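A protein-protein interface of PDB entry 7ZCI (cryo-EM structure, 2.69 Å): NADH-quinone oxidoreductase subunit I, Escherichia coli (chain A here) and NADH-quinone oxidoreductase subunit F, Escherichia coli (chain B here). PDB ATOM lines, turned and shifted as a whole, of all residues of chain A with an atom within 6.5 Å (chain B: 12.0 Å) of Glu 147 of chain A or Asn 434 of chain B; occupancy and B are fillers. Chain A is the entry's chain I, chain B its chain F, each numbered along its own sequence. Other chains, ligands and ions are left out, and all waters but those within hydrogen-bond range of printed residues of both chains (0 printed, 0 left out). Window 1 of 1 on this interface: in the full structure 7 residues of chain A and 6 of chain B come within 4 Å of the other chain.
NH2 of Arg 59 of chain A is in hydrogen-bond range of O of Tyr 145 of chain A, at 2.6 Å.
Among the printed residues, pairs that only touch across the chains: Tyr 145 of chain A with Gly 435 of chain B (3.4 Å), Tyr 145 of chain A with Ile 436 of chain B (3.6 Å), Pro 146 of chain A with Asn 434 of chain B (3.7 Å) and Glu 147 of chain A with Asn 434 of chain B (3.6 Å).
No residue of chain B comes within 4 Å of Pro 142 of chain A.
Of the printed residues of chain B, Tyr 145 of chain A touches Gly 435 and Ile 436.
Pro 146 of chain A touches just one residue of chain B: Asn 434 (3.7 Å).
Glu 147 of chain A touches just one residue of chain B: Asn 434 (3.6 Å).
No residue of chain B comes within 4 Å of Asn 149 of chain A.
Thr 430 of chain B touches none of the printed residues of chain A.
His 431 of chain B touches none of the printed residues of chain A.
Asn 434 of chain B touches two residues of chain A.
Printed residues of chain A within 4 Å of Gly 435 of chain B: Tyr 145 (3.4 Å).
Of the printed residues of chain A, Ile 436 of chain B touches Tyr 145 (3.6 Å).
The nearest residue of chain B that does not touch Glu 147 of chain A is Ile 433 of chain B (6.4 Å).
Hydrophobic or aromatic side chains of chain B within 4 Å of the printed part of chain A: Ile 436.
Of the 9 printed residues of chain A, 3 touch a printed residue of chain B.
Hydrophobic or aromatic side chains of chain A within 4 Å of the printed part of chain B: Tyr 145 and Pro 146.
Among the printed residues, 4 pairs touch across the chains.
Among the printed residues, no Asp or Glu carboxylate lies within 4 Å of a Lys or Arg side-chain nitrogen of the other chain.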
ATOM      1  N   PRO A  54      24.913 -16.663   2.742  1.00  0.00           N
ATOM      2  CA  PRO A  54      26.063 -17.563   2.968  1.00  0.00           C
ATOM      3  C   PRO A  54      27.117 -17.053   3.941  1.00  0.00           C
ATOM      4  O   PRO A  54      27.802 -17.871   4.566  1.00  0.00           O
ATOM      5  CB  PRO A  54      26.645 -17.727   1.561  1.00  0.00           C
ATOM      6  CG  PRO A  54      25.483 -17.612   0.682  1.00  0.00           C
ATOM      7  CD  PRO A  54      24.553 -16.621   1.310  1.00  0.00           C
ATOM      8  N   ARG A  59      19.236 -12.536   5.867  1.00  0.00           N
ATOM      9  CA  ARG A  59      19.002 -12.056   4.516  1.00  0.00           C
ATOM     10  C   ARG A  59      18.029 -10.889   4.471  1.00  0.00           C
ATOM     11  O   ARG A  59      18.082 -10.090   3.533  1.00  0.00           O
ATOM     12  CB  ARG A  59      18.477 -13.195   3.660  1.00  0.00           C
ATOM     13  CG  ARG A  59      19.500 -13.870   2.814  1.00  0.00           C
ATOM     14  CD  ARG A  59      18.829 -14.882   1.933  1.00  0.00           C
ATOM     15  NE  ARG A  59      19.762 -15.508   1.012  1.00  0.00           N
ATOM     16  CZ  ARG A  59      19.795 -16.806   0.762  1.00  0.00           C
ATOM     17  NH1 ARG A  59      18.963 -17.644   1.355  1.00  0.00           N
ATOM     18  NH2 ARG A  59      20.684 -17.274  -0.107  1.00  0.00           N
ATOM     19  N   PRO A 142      20.827 -21.046   4.733  1.00  0.00           N
ATOM     20  CA  PRO A 142      20.256 -20.372   3.560  1.00  0.00           C
ATOM     21  C   PRO A 142      18.948 -20.942   3.041  1.00  0.00           C
ATOM     22  O   PRO A 142      18.368 -20.341   2.130  1.00  0.00           O
ATOM     23  CB  PRO A 142      21.362 -20.519   2.514  1.00  0.00           C
ATOM     24  CG  PRO A 142      22.051 -21.752   2.890  1.00  0.00           C
ATOM     25  CD  PRO A 142      22.009 -21.844   4.378  1.00  0.00           C
ATOM     26  N   LYS A 144      16.227 -22.834   0.917  1.00  0.00           N
ATOM     27  CA  LYS A 144      16.082 -23.418  -0.411  1.00  0.00           C
ATOM     28  C   LYS A 144      16.907 -22.715  -1.477  1.00  0.00           C
ATOM     29  O   LYS A 144      17.092 -23.272  -2.559  1.00  0.00           O
ATOM     30  CB  LYS A 144      14.613 -23.403  -0.834  1.00  0.00           C
ATOM     31  CG  LYS A 144      13.697 -24.150   0.110  1.00  0.00           C
ATOM     32  CD  LYS A 144      12.302 -24.294  -0.459  1.00  0.00           C
ATOM     33  CE  LYS A 144      11.639 -22.956  -0.637  1.00  0.00           C
ATOM     34  NZ  LYS A 144      10.230 -23.093  -1.087  1.00  0.00           N
ATOM     35  N   TYR A 145      17.402 -21.509  -1.210  1.00  0.00           N
ATOM     36  CA  TYR A 145      18.215 -20.758  -2.164  1.00  0.00           C
ATOM     37  C   TYR A 145      19.583 -20.588  -1.524  1.00  0.00           C
ATOM     38  O   TYR A 145      19.803 -19.658  -0.735  1.00  0.00           O
ATOM     39  CB  TYR A 145      17.564 -19.424  -2.517  1.00  0.00           C
ATOM     40  CG  TYR A 145      16.130 -19.585  -2.959  1.00  0.00           C
ATOM     41  CD1 TYR A 145      15.828 -20.041  -4.228  1.00  0.00           C
ATOM     42  CD2 TYR A 145      15.083 -19.298  -2.099  1.00  0.00           C
ATOM     43  CE1 TYR A 145      14.525 -20.200  -4.630  1.00  0.00           C
ATOM     44  CE2 TYR A 145      13.776 -19.454  -2.494  1.00  0.00           C
ATOM     45  CZ  TYR A 145      13.503 -19.904  -3.758  1.00  0.00           C
ATOM     46  OH  TYR A 145      12.199 -20.059  -4.154  1.00  0.00           O
ATOM     47  N   PRO A 146      20.538 -21.462  -1.845  1.00  0.00           N
ATOM     48  CA  PRO A 146      21.722 -21.606  -0.992  1.00  0.00           C
ATOM     49  C   PRO A 146      22.781 -20.535  -1.153  1.00  0.00           C
ATOM     50  O   PRO A 146      23.649 -20.432  -0.278  1.00  0.00           O
ATOM     51  CB  PRO A 146      22.274 -22.974  -1.402  1.00  0.00           C
ATOM     52  CG  PRO A 146      21.843 -23.128  -2.808  1.00  0.00           C
ATOM     53  CD  PRO A 146      20.503 -22.471  -2.914  1.00  0.00           C
ATOM     54  N   GLU A 147      22.764 -19.744  -2.220  1.00  0.00           N
ATOM     55  CA  GLU A 147      23.881 -18.851  -2.476  1.00  0.00           C
ATOM     56  C   GLU A 147      23.525 -17.398  -2.738  1.00  0.00           C
ATOM     57  O   GLU A 147      24.448 -16.589  -2.859  1.00  0.00           O
ATOM     58  CB  GLU A 147      24.706 -19.358  -3.665  1.00  0.00           C
ATOM     59  CG  GLU A 147      25.850 -20.261  -3.270  1.00  0.00           C
ATOM     60  CD  GLU A 147      25.842 -21.568  -4.029  1.00  0.00           C
ATOM     61  OE1 GLU A 147      25.567 -21.546  -5.246  1.00  0.00           O
ATOM     62  OE2 GLU A 147      26.118 -22.618  -3.410  1.00  0.00           O
ATOM     63  N   TYR A 148      22.250 -17.031  -2.835  1.00  0.00           N
ATOM     64  CA  TYR A 148      21.927 -15.662  -3.211  1.00  0.00           C
ATOM     65  C   TYR A 148      22.206 -14.712  -2.058  1.00  0.00           C
ATOM     66  O   TYR A 148      21.815 -14.961  -0.914  1.00  0.00           O
ATOM     67  CB  TYR A 148      20.475 -15.530  -3.658  1.00  0.00           C
ATOM     68  CG  TYR A 148      20.183 -14.157  -4.215  1.00  0.00           C
ATOM     69  CD1 TYR A 148      20.695 -13.771  -5.443  1.00  0.00           C
ATOM     70  CD2 TYR A 148      19.430 -13.238  -3.504  1.00  0.00           C
ATOM     71  CE1 TYR A 148      20.454 -12.524  -5.953  1.00  0.00           C
ATOM     72  CE2 TYR A 148      19.188 -11.982  -4.006  1.00  0.00           C
ATOM     73  CZ  TYR A 148      19.697 -11.635  -5.233  1.00  0.00           C
ATOM     74  OH  TYR A 148      19.458 -10.384  -5.744  1.00  0.00           O
ATOM     75  N   ASN A 149      22.913 -13.636  -2.365  1.00  0.00           N
ATOM     76  CA  ASN A 149      23.204 -12.562  -1.428  1.00  0.00           C
ATOM     77  C   ASN A 149      22.734 -11.281  -2.091  1.00  0.00           C
ATOM     78  O   ASN A 149      23.312 -10.859  -3.096  1.00  0.00           O
ATOM     79  CB  ASN A 149      24.694 -12.505  -1.106  1.00  0.00           C
ATOM     80  CG  ASN A 149      24.993 -11.744   0.155  1.00  0.00           C
ATOM     81  OD1 ASN A 149      24.197 -10.929   0.611  1.00  0.00           O
ATOM     82  ND2 ASN A 149      26.160 -11.990   0.721  1.00  0.00           N
ATOM     83  N   THR B 430      22.981 -12.448 -17.407  1.00  0.00           N
ATOM     84  CA  THR B 430      22.455 -13.095 -16.218  1.00  0.00           C
ATOM     85  C   THR B 430      23.382 -14.229 -15.816  1.00  0.00           C
ATOM     86  O   THR B 430      23.847 -14.990 -16.666  1.00  0.00           O
ATOM     87  CB  THR B 430      21.052 -13.666 -16.463  1.00  0.00           C
ATOM     88  OG1 THR B 430      21.046 -14.398 -17.693  1.00  0.00           O
ATOM     89  CG2 THR B 430      20.028 -12.573 -16.555  1.00  0.00           C
ATOM     90  N   HIS B 431      23.652 -14.340 -14.526  1.00  0.00           N
ATOM     91  CA  HIS B 431      24.264 -15.536 -13.980  1.00  0.00           C
ATOM     92  C   HIS B 431      23.184 -16.424 -13.380  1.00  0.00           C
ATOM     93  O   HIS B 431      22.037 -16.017 -13.191  1.00  0.00           O
ATOM     94  CB  HIS B 431      25.326 -15.188 -12.939  1.00  0.00           C
ATOM     95  CG  HIS B 431      24.784 -14.481 -11.743  1.00  0.00           C
ATOM     96  ND1 HIS B 431      24.764 -13.109 -11.647  1.00  0.00           N
ATOM     97  CD2 HIS B 431      24.257 -14.948 -10.587  1.00  0.00           C
ATOM     98  CE1 HIS B 431      24.235 -12.760 -10.490  1.00  0.00           C
ATOM     99  NE2 HIS B 431      23.921 -13.856  -9.826  1.00  0.00           N
ATOM    100  N   LEU B 432      23.558 -17.662 -13.095  1.00  0.00           N
ATOM    101  CA  LEU B 432      22.601 -18.637 -12.604  1.00  0.00           C
ATOM    102  C   LEU B 432      22.384 -18.454 -11.108  1.00  0.00           C
ATOM    103  O   LEU B 432      23.340 -18.292 -10.346  1.00  0.00           O
ATOM    104  CB  LEU B 432      23.082 -20.057 -12.901  1.00  0.00           C
ATOM    105  CG  LEU B 432      22.614 -20.723 -14.202  1.00  0.00           C
ATOM    106  CD1 LEU B 432      21.110 -20.915 -14.192  1.00  0.00           C
ATOM    107  CD2 LEU B 432      23.042 -19.964 -15.444  1.00  0.00           C
ATOM    108  N   ILE B 433      21.124 -18.464 -10.697  1.00  0.00           N
ATOM    109  CA  ILE B 433      20.743 -18.485  -9.292  1.00  0.00           C
ATOM    110  C   ILE B 433      20.232 -19.883  -8.991  1.00  0.00           C
ATOM    111  O   ILE B 433      19.453 -20.442  -9.772  1.00  0.00           O
ATOM    112  CB  ILE B 433      19.698 -17.400  -8.984  1.00  0.00           C
ATOM    113  CG1 ILE B 433      20.288 -16.031  -9.307  1.00  0.00           C
ATOM    114  CG2 ILE B 433      19.275 -17.442  -7.534  1.00  0.00           C
ATOM    115  CD1 ILE B 433      19.327 -14.922  -9.190  1.00  0.00           C
ATOM    116  N   ASN B 434      20.685 -20.449  -7.870  1.00  0.00           N
ATOM    117  CA  ASN B 434      20.671 -21.897  -7.689  1.00  0.00           C
ATOM    118  C   ASN B 434      19.257 -22.463  -7.608  1.00  0.00           C
ATOM    119  O   ASN B 434      18.916 -23.403  -8.334  1.00  0.00           O
ATOM    120  CB  ASN B 434      21.468 -22.261  -6.444  1.00  0.00           C
ATOM    121  CG  ASN B 434      21.999 -23.665  -6.489  1.00  0.00           C
ATOM    122  OD1 ASN B 434      21.273 -24.621  -6.235  1.00  0.00           O
ATOM    123  ND2 ASN B 434      23.273 -23.802  -6.820  1.00  0.00           N
ATOM    124  N   GLY B 435      18.417 -21.902  -6.756  1.00  0.00           N
ATOM    125  CA  GLY B 435      17.102 -22.475  -6.581  1.00  0.00           C
ATOM    126  C   GLY B 435      16.032 -21.967  -7.519  1.00  0.00           C
ATOM    127  O   GLY B 435      14.857 -22.279  -7.313  1.00  0.00           O
ATOM    128  N   ILE B 436      16.389 -21.202  -8.545  1.00  0.00           N
ATOM    129  CA  ILE B 436      15.419 -20.543  -9.410  1.00  0.00           C
ATOM    130  C   ILE B 436      15.674 -20.964 -10.848  1.00  0.00           C
ATOM    131  O   ILE B 436      16.743 -20.680 -11.402  1.00  0.00           O
ATOM    132  CB  ILE B 436      15.484 -19.016  -9.269  1.00  0.00           C
ATOM    133  CG1 ILE B 436      15.115 -18.604  -7.846  1.00  0.00           C
ATOM    134  CG2 ILE B 436      14.565 -18.351 -10.268  1.00  0.00           C
ATOM    135  CD1 ILE B 436      15.481 -17.203  -7.505  1.00  0.00           C
ATOM    136  N   GLN B 437      14.694 -21.621 -11.454  1.00  0.00           N
ATOM    137  CA  GLN B 437      14.777 -21.998 -12.860  1.00  0.00           C
ATOM    138  C   GLN B 437      14.520 -20.781 -13.737  1.00  0.00           C
ATOM    139  O   GLN B 437      13.503 -20.105 -13.561  1.00  0.00           O
ATOM    140  CB  GLN B 437      13.765 -23.083 -13.187  1.00  0.00           C
ATOM    141  CG  GLN B 437      13.995 -24.388 -12.464  1.00  0.00           C
ATOM    142  CD  GLN B 437      12.830 -25.338 -12.609  1.00  0.00           C
ATOM    143  OE1 GLN B 437      11.864 -25.269 -11.857  1.00  0.00           O
ATOM    144  NE2 GLN B 437      12.914 -26.228 -13.585  1.00  0.00           N
ATOM    145  N   PRO B 438      15.407 -20.473 -14.679  1.00  0.00           N
ATOM    146  CA  PRO B 438      15.235 -19.260 -15.480  1.00  0.00           C
ATOM    147  C   PRO B 438      14.113 -19.380 -16.497  1.00  0.00           C
ATOM    148  O   PRO B 438      13.762 -20.469 -16.954  1.00  0.00           O
ATOM    149  CB  PRO B 438      16.592 -19.103 -16.172  1.00  0.00           C
ATOM    150  CG  PRO B 438      17.130 -20.473 -16.236  1.00  0.00           C
ATOM    151  CD  PRO B 438      16.650 -21.184 -15.012  1.00  0.00           C
ATOM    152  N   ASN B 439      13.551 -18.228 -16.847  1.00  0.00           N
ATOM    153  CA  ASN B 439      12.550 -18.124 -17.902  1.00  0.00           C
ATOM    154  C   ASN B 439      13.282 -18.122 -19.236  1.00  0.00           C
ATOM    155  O   ASN B 439      13.852 -17.111 -19.644  1.00  0.00           O
ATOM    156  CB  ASN B 439      11.716 -16.862 -17.721  1.00  0.00           C
ATOM    157  CG  ASN B 439      10.404 -16.919 -18.460  1.00  0.00           C
ATOM    158  OD1 ASN B 439       9.749 -17.950 -18.496  1.00  0.00           O
ATOM    159  ND2 ASN B 439      10.017 -15.809 -19.062  1.00  0.00           N
